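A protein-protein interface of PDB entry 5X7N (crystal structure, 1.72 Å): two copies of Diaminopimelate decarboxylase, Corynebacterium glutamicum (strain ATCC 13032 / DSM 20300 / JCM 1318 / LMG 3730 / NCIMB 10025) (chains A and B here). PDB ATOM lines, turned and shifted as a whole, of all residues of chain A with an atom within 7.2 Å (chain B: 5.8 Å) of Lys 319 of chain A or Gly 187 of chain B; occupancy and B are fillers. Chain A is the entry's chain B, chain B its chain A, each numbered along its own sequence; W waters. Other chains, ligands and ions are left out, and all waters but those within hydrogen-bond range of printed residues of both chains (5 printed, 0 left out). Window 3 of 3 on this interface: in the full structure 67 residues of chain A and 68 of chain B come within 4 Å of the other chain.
The side-chain carboxylate (OD2) of Asp 140 of chain B is in salt-bridge range of the side-chain amino group (NZ) of Lys 319 of chain A. The side-chain amide oxygen of Gln 143 of chain B lies within hydrogen-bond range of the backbone NH of Thr 318 of chain A (3.0 Å). N of Gln 184 of chain B lies within hydrogen-bond range of OH of Tyr 331 of chain A (3.3 Å). O of Lys 185 of chain B lies within hydrogen-bond range of NZ of Lys 319 of chain A (2.9 Å). The backbone carbonyl oxygen of Gly 187 of chain B lies within hydrogen-bond range of the side-chain amino group of Lys 319 of chain A, 2.8 Å away.
OD1 of Asp 140 of chain B is in hydrogen-bond range of N of Gly 187 of chain B, at 3.0 Å. The backbone NH (N) of Lys 166 of chain B is in hydrogen-bond range of the backbone carbonyl oxygen (O) of Phe 188 of chain B. O of Thr 317 of chain A lies within hydrogen-bond range of N of Ala 333 of chain A, at 2.9 Å. The backbone carbonyl oxygen (O) of Lys 319 of chain A is in hydrogen-bond range of the backbone NH (N) of Tyr 331 of chain A (2.8 Å). O of Val 321 of chain A is in hydrogen-bond range of N of Arg 329 of chain A (2.8 Å). The guanidinium group (NH1) of Arg 368 of chain A is in hydrogen-bond range of the side-chain hydroxyl (OH) of Tyr 331 of chain A, at 3.1 Å.
Among the printed residues, pairs that only touch across the chains: Thr 317 of chain A with Ser 141 of chain B (3.7 Å), Thr 317 of chain A with Gln 143 of chain B (3.5 Å), Lys 319 of chain A with Phe 186 of chain B (3.5 Å), Val 321 of chain A with Lys 166 of chain B (3.6 Å), Val 321 of chain A with Gln 184 of chain B (3.9 Å) and Tyr 331 of chain A with Lys 185 of chain B (3.6 Å).
Gly 187 of chain B touches one residue of chain A. Printed residues of chain A within 4 Å of Asp 140 of chain B: Lys 319 (2.8 Å). Printed residues of chain A within 4 Å of Lys 166 of chain B: Val 321. Printed residues of chain A within 4 Å of Gln 143 of chain B: Thr 317 and Thr 318. Of the printed residues of chain B, Thr 318 of chain A touches Gln 143. Of the printed residues of chain B, Tyr 331 of chain A touches Gln 184 (3.3 Å) and Lys 185 (3.6 Å). Arg 329 of chain A touches none of the printed residues of chain B. The nearest printed residue of chain B that does not touch Thr 317 of chain A is Asp 140 of chain B (6.0 Å).
Printed residues of chain B that touch a printed residue of chain A: Asp 140, Ser 141, Gln 143, Lys 166, Gln 184, Lys 185, Phe 186 and Gly 187. Printed residues of chain A that touch a printed residue of chain B: Thr 317, Thr 318, Lys 319, Val 321 and Tyr 331. Among the printed residues, 11 pairs touch across the chains. Among the printed residues, Asp or Glu carboxylates within 4 Å of a Lys or Arg side-chain nitrogen of the other chain: Lys 319 of chain A with Asp 140 of chain B (3.6 Å).
No position is printed for both chains. Of the 11 pairs that touch across the chains among the printed residues, none has its exchanged pair printed and touching as well.
Water W3 lies within hydrogen-bond range of OG1 of Thr 317 of chain A and OG of Ser 141 of chain B. Water W5 bridges the side-chain carboxylate (OD2) of Asp 140 of chain B (2.6 Å) and the side-chain amino group (NZ) of Lys 319 of chain A (3.1 Å). Water W2 lies within hydrogen-bond range of O of Gly 316 of chain A, OG1 of Thr 318 of chain A and NE2 of Gln 143 of chain B. Water W1 lies within hydrogen-bond range of the side-chain amide oxygen (OE1) of Gln 143 of chain B (2.9 Å) and the backbone carbonyl oxygen (O) of Thr 318 of chain A (3.3 Å). Water W4 lies within hydrogen-bond range of the backbone carbonyl oxygen (O) of Thr 318 of chain A (3.0 Å) and the side-chain amide oxygen (OE1) of Gln 143 of chain B (3.3 Å).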
ATOM      1  N   GLY A 316      19.151  30.905 -14.548  1.00  0.00           N
ATOM      2  CA  GLY A 316      20.461  30.323 -14.693  1.00  0.00           C
ATOM      3  C   GLY A 316      20.628  29.702 -16.106  1.00  0.00           C
ATOM      4  O   GLY A 316      20.495  30.368 -17.164  1.00  0.00           O
ATOM      5  N   THR A 317      20.853  28.385 -16.132  1.00  0.00           N
ATOM      6  CA  THR A 317      21.138  27.624 -17.317  1.00  0.00           C
ATOM      7  C   THR A 317      20.040  27.667 -18.336  1.00  0.00           C
ATOM      8  O   THR A 317      18.872  27.526 -17.985  1.00  0.00           O
ATOM      9  CB  THR A 317      21.444  26.167 -16.949  1.00  0.00           C
ATOM     10  OG1 THR A 317      22.505  26.136 -15.994  1.00  0.00           O
ATOM     11  CG2 THR A 317      21.779  25.341 -18.163  1.00  0.00           C
ATOM     12  N   THR A 318      20.394  27.906 -19.603  1.00  0.00           N
ATOM     13  CA  THR A 318      19.470  27.786 -20.689  1.00  0.00           C
ATOM     14  C   THR A 318      20.001  26.780 -21.703  1.00  0.00           C
ATOM     15  O   THR A 318      21.202  26.756 -21.962  1.00  0.00           O
ATOM     16  CB  THR A 318      19.157  29.120 -21.374  1.00  0.00           C
ATOM     17  OG1 THR A 318      20.375  29.790 -21.700  1.00  0.00           O
ATOM     18  CG2 THR A 318      18.392  30.011 -20.312  1.00  0.00           C
ATOM     19  N   LYS A 319      19.085  26.025 -22.271  1.00  0.00           N
ATOM     20  CA  LYS A 319      19.420  25.037 -23.247  1.00  0.00           C
ATOM     21  C   LYS A 319      18.284  24.705 -24.165  1.00  0.00           C
ATOM     22  O   LYS A 319      17.144  24.611 -23.748  1.00  0.00           O
ATOM     23  CB  LYS A 319      20.107  23.807 -22.630  1.00  0.00           C
ATOM     24  CG  LYS A 319      19.260  22.938 -21.787  1.00  0.00           C
ATOM     25  CD  LYS A 319      19.924  21.534 -21.606  1.00  0.00           C
ATOM     26  CE  LYS A 319      21.011  21.497 -20.561  1.00  0.00           C
ATOM     27  NZ  LYS A 319      21.213  20.140 -19.978  1.00  0.00           N
ATOM     28  N   ASP A 320      18.635  24.495 -25.460  1.00  0.00           N
ATOM     29  CA  ASP A 320      17.693  24.010 -26.420  1.00  0.00           C
ATOM     30  C   ASP A 320      17.684  22.528 -26.469  1.00  0.00           C
ATOM     31  O   ASP A 320      18.765  21.943 -26.590  1.00  0.00           O
ATOM     32  CB  ASP A 320      18.094  24.536 -27.803  1.00  0.00           C
ATOM     33  CG  ASP A 320      17.738  25.988 -27.985  1.00  0.00           C
ATOM     34  OD1 ASP A 320      16.840  26.541 -27.335  1.00  0.00           O
ATOM     35  OD2 ASP A 320      18.387  26.576 -28.826  1.00  0.00           O
ATOM     36  N   VAL A 321      16.486  21.930 -26.355  1.00  0.00           N
ATOM     37  CA  VAL A 321      16.327  20.461 -26.311  1.00  0.00           C
ATOM     38  C   VAL A 321      15.399  20.033 -27.451  1.00  0.00           C
ATOM     39  O   VAL A 321      14.227  20.432 -27.547  1.00  0.00           O
ATOM     40  CB  VAL A 321      15.710  20.023 -24.949  1.00  0.00           C
ATOM     41  CG1 VAL A 321      15.401  18.511 -24.939  1.00  0.00           C
ATOM     42  CG2 VAL A 321      16.602  20.379 -23.831  1.00  0.00           C
ATOM     43  N   THR A 328      11.791  21.935 -31.061  1.00  0.00           N
ATOM     44  CA  THR A 328      12.754  22.209 -30.008  1.00  0.00           C
ATOM     45  C   THR A 328      11.987  22.839 -28.833  1.00  0.00           C
ATOM     46  O   THR A 328      11.064  23.563 -29.067  1.00  0.00           O
ATOM     47  CB  THR A 328      13.779  23.173 -30.586  1.00  0.00           C
ATOM     48  OG1 THR A 328      14.447  22.507 -31.639  1.00  0.00           O
ATOM     49  CG2 THR A 328      14.781  23.629 -29.586  1.00  0.00           C
ATOM     50  N   ARG A 329      12.303  22.462 -27.596  1.00  0.00           N
ATOM     51  CA  ARG A 329      11.813  23.112 -26.430  1.00  0.00           C
ATOM     52  C   ARG A 329      12.970  23.818 -25.718  1.00  0.00           C
ATOM     53  O   ARG A 329      14.034  23.208 -25.452  1.00  0.00           O
ATOM     54  CB  ARG A 329      11.241  22.090 -25.535  1.00  0.00           C
ATOM     55  CG  ARG A 329      10.348  22.717 -24.488  1.00  0.00           C
ATOM     56  CD  ARG A 329       9.817  21.708 -23.458  1.00  0.00           C
ATOM     57  NE  ARG A 329       9.252  20.475 -23.998  1.00  0.00           N
ATOM     58  CZ  ARG A 329       8.022  20.428 -24.525  1.00  0.00           C
ATOM     59  NH1 ARG A 329       7.236  21.520 -24.675  1.00  0.00           N
ATOM     60  NH2 ARG A 329       7.562  19.263 -24.956  1.00  0.00           N
ATOM     61  N   ARG A 330      12.790  25.107 -25.369  1.00  0.00           N
ATOM     62  CA  ARG A 330      13.841  25.857 -24.734  1.00  0.00           C
ATOM     63  C   ARG A 330      13.688  25.703 -23.199  1.00  0.00           C
ATOM     64  O   ARG A 330      12.649  26.075 -22.665  1.00  0.00           O
ATOM     65  CB  ARG A 330      13.815  27.380 -25.156  1.00  0.00           C
ATOM     66  CG  ARG A 330      15.024  28.156 -24.661  1.00  0.00           C
ATOM     67  CD  ARG A 330      15.175  29.501 -25.376  1.00  0.00           C
ATOM     68  NE  ARG A 330      16.450  30.091 -24.997  1.00  0.00           N
ATOM     69  CZ  ARG A 330      16.625  30.979 -23.999  1.00  0.00           C
ATOM     70  NH1 ARG A 330      15.606  31.465 -23.277  1.00  0.00           N
ATOM     71  NH2 ARG A 330      17.856  31.431 -23.744  1.00  0.00           N
ATOM     72  N   TYR A 331      14.691  25.135 -22.557  1.00  0.00           N
ATOM     73  CA  TYR A 331      14.676  24.839 -21.105  1.00  0.00           C
ATOM     74  C   TYR A 331      15.365  25.984 -20.438  1.00  0.00           C
ATOM     75  O   TYR A 331      16.548  26.255 -20.690  1.00  0.00           O
ATOM     76  CB  TYR A 331      15.389  23.542 -20.755  1.00  0.00           C
ATOM     77  CG  TYR A 331      14.455  22.303 -20.867  1.00  0.00           C
ATOM     78  CD1 TYR A 331      14.050  21.811 -22.112  1.00  0.00           C
ATOM     79  CD2 TYR A 331      13.948  21.688 -19.750  1.00  0.00           C
ATOM     80  CE1 TYR A 331      13.245  20.713 -22.235  1.00  0.00           C
ATOM     81  CE2 TYR A 331      13.120  20.572 -19.859  1.00  0.00           C
ATOM     82  CZ  TYR A 331      12.728  20.101 -21.084  1.00  0.00           C
ATOM     83  OH  TYR A 331      11.913  18.994 -21.173  1.00  0.00           O
ATOM     84  N   ILE A 332      14.646  26.631 -19.514  1.00  0.00           N
ATOM     85  CA  ILE A 332      15.244  27.670 -18.650  1.00  0.00           C
ATOM     86  C   ILE A 332      15.209  27.181 -17.204  1.00  0.00           C
ATOM     87  O   ILE A 332      14.124  26.929 -16.701  1.00  0.00           O
ATOM     88  CB  ILE A 332      14.471  29.023 -18.773  1.00  0.00           C
ATOM     89  CG1 ILE A 332      14.331  29.440 -20.258  1.00  0.00           C
ATOM     90  CG2 ILE A 332      15.065  30.114 -17.886  1.00  0.00           C
ATOM     91  CD1 ILE A 332      13.552  30.725 -20.440  1.00  0.00           C
ATOM     92  N   ALA A 333      16.381  27.129 -16.560  1.00  0.00           N
ATOM     93  CA  ALA A 333      16.504  26.785 -15.177  1.00  0.00           C
ATOM     94  C   ALA A 333      16.455  28.018 -14.329  1.00  0.00           C
ATOM     95  O   ALA A 333      17.096  29.029 -14.664  1.00  0.00           O
ATOM     96  CB  ALA A 333      17.779  26.024 -14.911  1.00  0.00           C
ATOM     97  N   ARG A 368      10.102  25.816 -21.410  1.00  0.00           N
ATOM     98  CA  ARG A 368       9.758  25.122 -20.199  1.00  0.00           C
ATOM     99  C   ARG A 368      10.672  25.712 -19.108  1.00  0.00           C
ATOM    100  O   ARG A 368      11.895  25.812 -19.305  1.00  0.00           O
ATOM    101  CB  ARG A 368       9.997  23.618 -20.370  1.00  0.00           C
ATOM    102  CG  ARG A 368       9.735  22.805 -19.068  1.00  0.00           C
ATOM    103  CD  ARG A 368       9.567  21.333 -19.327  1.00  0.00           C
ATOM    104  NE  ARG A 368       8.344  21.072 -20.062  1.00  0.00           N
ATOM    105  CZ  ARG A 368       8.023  19.928 -20.679  1.00  0.00           C
ATOM    106  NH1 ARG A 368       8.849  18.862 -20.659  1.00  0.00           N
ATOM    107  NH2 ARG A 368       6.882  19.867 -21.354  1.00  0.00           N
ATOM    108  N   LEU B 139      29.128  17.256 -15.421  1.00  0.00           N
ATOM    109  CA  LEU B 139      28.731  18.404 -16.184  1.00  0.00           C
ATOM    110  C   LEU B 139      27.410  18.147 -16.897  1.00  0.00           C
ATOM    111  O   LEU B 139      27.210  17.189 -17.601  1.00  0.00           O
ATOM    112  CB  LEU B 139      29.782  18.757 -17.245  1.00  0.00           C
ATOM    113  CG  LEU B 139      31.139  19.182 -16.704  1.00  0.00           C
ATOM    114  CD1 LEU B 139      32.139  19.238 -17.866  1.00  0.00           C
ATOM    115  CD2 LEU B 139      31.043  20.636 -16.187  1.00  0.00           C
ATOM    116  N   ASP B 140      26.528  19.104 -16.712  1.00  0.00           N
ATOM    117  CA  ASP B 140      25.172  19.054 -17.252  1.00  0.00           C
ATOM    118  C   ASP B 140      24.896  19.982 -18.413  1.00  0.00           C
ATOM    119  O   ASP B 140      23.869  19.801 -19.108  1.00  0.00           O
ATOM    120  CB  ASP B 140      24.185  19.311 -16.116  1.00  0.00           C
ATOM    121  CG  ASP B 140      22.881  18.509 -16.298  1.00  0.00           C
ATOM    122  OD1 ASP B 140      22.934  17.264 -16.274  1.00  0.00           O
ATOM    123  OD2 ASP B 140      21.891  19.115 -16.623  1.00  0.00           O
ATOM    124  N   SER B 141      25.743  20.981 -18.657  1.00  0.00           N
ATOM    125  CA  SER B 141      25.481  21.942 -19.744  1.00  0.00           C
ATOM    126  C   SER B 141      26.758  22.631 -20.237  1.00  0.00           C
ATOM    127  O   SER B 141      27.807  22.585 -19.630  1.00  0.00           O
ATOM    128  CB  SER B 141      24.577  23.105 -19.293  1.00  0.00           C
ATOM    129  OG  SER B 141      25.260  23.979 -18.352  1.00  0.00           O
ATOM    130  N   GLN B 143      27.235  25.795 -20.571  1.00  0.00           N
ATOM    131  CA  GLN B 143      27.540  26.922 -19.678  1.00  0.00           C
ATOM    132  C   GLN B 143      28.283  26.458 -18.496  1.00  0.00           C
ATOM    133  O   GLN B 143      29.230  27.096 -18.074  1.00  0.00           O
ATOM    134  CB  GLN B 143      26.245  27.702 -19.294  1.00  0.00           C
ATOM    135  CG  GLN B 143      25.660  28.553 -20.386  1.00  0.00           C
ATOM    136  CD  GLN B 143      24.230  29.007 -20.004  1.00  0.00           C
ATOM    137  OE1 GLN B 143      23.312  28.207 -19.984  1.00  0.00           O
ATOM    138  NE2 GLN B 143      24.073  30.290 -19.634  1.00  0.00           N
ATOM    139  N   ARG B 164      27.229  14.284 -18.376  1.00  0.00           N
ATOM    140  CA  ARG B 164      25.916  13.636 -18.445  1.00  0.00           C
ATOM    141  C   ARG B 164      25.368  13.625 -19.864  1.00  0.00           C
ATOM    142  O   ARG B 164      25.148  14.651 -20.486  1.00  0.00           O
ATOM    143  CB  ARG B 164      24.928  14.248 -17.517  1.00  0.00           C
ATOM    144  CG  ARG B 164      23.601  13.373 -17.550  1.00  0.00           C
ATOM    145  CD  ARG B 164      22.813  13.640 -16.350  1.00  0.00           C
ATOM    146  NE  ARG B 164      21.596  12.848 -16.377  1.00  0.00           N
ATOM    147  CZ  ARG B 164      20.667  12.950 -15.420  1.00  0.00           C
ATOM    148  NH1 ARG B 164      20.817  13.725 -14.390  1.00  0.00           N
ATOM    149  NH2 ARG B 164      19.632  12.201 -15.472  1.00  0.00           N
ATOM    150  N   VAL B 165      25.092  12.430 -20.382  1.00  0.00           N
ATOM    151  CA  VAL B 165      24.537  12.228 -21.659  1.00  0.00           C
ATOM    152  C   VAL B 165      23.149  11.563 -21.574  1.00  0.00           C
ATOM    153  O   VAL B 165      22.889  10.837 -20.658  1.00  0.00           O
ATOM    154  CB  VAL B 165      25.410  11.319 -22.455  1.00  0.00           C
ATOM    155  CG1 VAL B 165      24.815  11.019 -23.767  1.00  0.00           C
ATOM    156  CG2 VAL B 165      26.776  12.013 -22.654  1.00  0.00           C
ATOM    157  N   LYS B 166      22.290  11.909 -22.523  1.00  0.00           N
ATOM    158  CA  LYS B 166      20.910  11.312 -22.591  1.00  0.00           C
ATOM    159  C   LYS B 166      20.919  10.258 -23.718  1.00  0.00           C
ATOM    160  O   LYS B 166      20.996  10.631 -24.944  1.00  0.00           O
ATOM    161  CB  LYS B 166      19.885  12.412 -22.931  1.00  0.00           C
ATOM    162  CG  LYS B 166      19.713  13.503 -21.891  1.00  0.00           C
ATOM    163  CD  LYS B 166      18.628  14.530 -22.302  1.00  0.00           C
ATOM    164  CE  LYS B 166      19.058  15.346 -23.471  1.00  0.00           C
ATOM    165  NZ  LYS B 166      17.930  16.236 -23.841  1.00  0.00           N
ATOM    166  N   GLN B 184      13.856  16.331 -21.551  1.00  0.00           N
ATOM    167  CA  GLN B 184      14.107  16.632 -20.134  1.00  0.00           C
ATOM    168  C   GLN B 184      15.313  17.552 -20.021  1.00  0.00           C
ATOM    169  O   GLN B 184      16.043  17.770 -20.973  1.00  0.00           O
ATOM    170  CB  GLN B 184      14.254  15.379 -19.330  1.00  0.00           C
ATOM    171  CG  GLN B 184      15.145  14.332 -19.957  1.00  0.00           C
ATOM    172  CD  GLN B 184      16.372  14.138 -19.184  1.00  0.00           C
ATOM    173  OE1 GLN B 184      16.788  15.061 -18.499  1.00  0.00           O
ATOM    174  NE2 GLN B 184      17.006  12.926 -19.275  1.00  0.00           N
ATOM    175  N   LYS B 185      15.479  18.098 -18.833  1.00  0.00           N
ATOM    176  CA  LYS B 185      16.442  19.212 -18.650  1.00  0.00           C
ATOM    177  C   LYS B 185      17.888  18.835 -18.546  1.00  0.00           C
ATOM    178  O   LYS B 185      18.735  19.714 -18.627  1.00  0.00           O
ATOM    179  CB  LYS B 185      16.015  19.948 -17.391  1.00  0.00           C
ATOM    180  CG  LYS B 185      16.273  19.235 -16.095  1.00  0.00           C
ATOM    181  CD  LYS B 185      15.706  20.105 -14.969  1.00  0.00           C
ATOM    182  CE  LYS B 185      15.929  19.476 -13.637  1.00  0.00           C
ATOM    183  NZ  LYS B 185      15.348  20.233 -12.510  1.00  0.00           N
ATOM    184  N   PHE B 186      18.203  17.545 -18.289  1.00  0.00           N
ATOM    185  CA  PHE B 186      19.533  17.137 -17.918  1.00  0.00           C
ATOM    186  C   PHE B 186      20.406  16.818 -19.110  1.00  0.00           C
ATOM    187  O   PHE B 186      19.942  16.360 -20.121  1.00  0.00           O
ATOM    188  CB  PHE B 186      19.496  15.851 -17.060  1.00  0.00           C
ATOM    189  CG  PHE B 186      18.759  15.986 -15.784  1.00  0.00           C
ATOM    190  CD1 PHE B 186      19.246  16.765 -14.775  1.00  0.00           C
ATOM    191  CD2 PHE B 186      17.525  15.352 -15.610  1.00  0.00           C
ATOM    192  CE1 PHE B 186      18.563  16.921 -13.569  1.00  0.00           C
ATOM    193  CE2 PHE B 186      16.824  15.509 -14.396  1.00  0.00           C
ATOM    194  CZ  PHE B 186      17.376  16.262 -13.368  1.00  0.00           C
ATOM    195  N   GLY B 187      21.651  17.192 -18.992  1.00  0.00           N
ATOM    196  CA  GLY B 187      22.697  16.620 -19.880  1.00  0.00           C
ATOM    197  C   GLY B 187      22.623  17.042 -21.325  1.00  0.00           C
ATOM    198  O   GLY B 187      22.026  18.081 -21.685  1.00  0.00           O
ATOM    199  N   PHE B 188      23.340  16.234 -22.140  1.00  0.00           N
ATOM    200  CA  PHE B 188      23.529  16.494 -23.527  1.00  0.00           C
ATOM    201  C   PHE B 188      23.006  15.273 -24.312  1.00  0.00           C
ATOM    202  O   PHE B 188      23.245  14.136 -23.936  1.00  0.00           O
ATOM    203  CB  PHE B 188      25.002  16.609 -23.847  1.00  0.00           C
ATOM    204  CG  PHE B 188      25.732  17.715 -23.076  1.00  0.00           C
ATOM    205  CD1 PHE B 188      26.249  17.538 -21.841  1.00  0.00           C
ATOM    206  CD2 PHE B 188      25.912  18.963 -23.696  1.00  0.00           C
ATOM    207  CE1 PHE B 188      26.907  18.545 -21.178  1.00  0.00           C
ATOM    208  CE2 PHE B 188      26.613  19.963 -23.037  1.00  0.00           C
ATOM    209  CZ  PHE B 188      27.155  19.766 -21.805  1.00  0.00           C
ATOM    210  N   SER B 189      22.341  15.561 -25.403  1.00  0.00           N
ATOM    211  CA  SER B 189      21.808  14.597 -26.308  1.00  0.00           C
ATOM    212  C   SER B 189      22.934  13.755 -26.952  1.00  0.00           C
ATOM    213  O   SER B 189      23.856  14.300 -27.546  1.00  0.00           O
ATOM    214  CB  SER B 189      20.981  15.252 -27.397  1.00  0.00           C
ATOM    215  OG  SER B 189      20.631  14.311 -28.363  1.00  0.00           O
HETATM  216  O   HOH W   1      24.264  25.795 -21.282  1.00  0.00           O
HETATM  217  O   HOH W   2      21.417  31.200 -19.544  1.00  0.00           O
HETATM  218  O   HOH W   3      24.370  24.450 -15.874  1.00  0.00           O
HETATM  219  O   HOH W   4      22.828  28.937 -23.135  1.00  0.00           O
HETATM  220  O   HOH W   5      21.593  21.609 -17.325  1.00  0.00           O
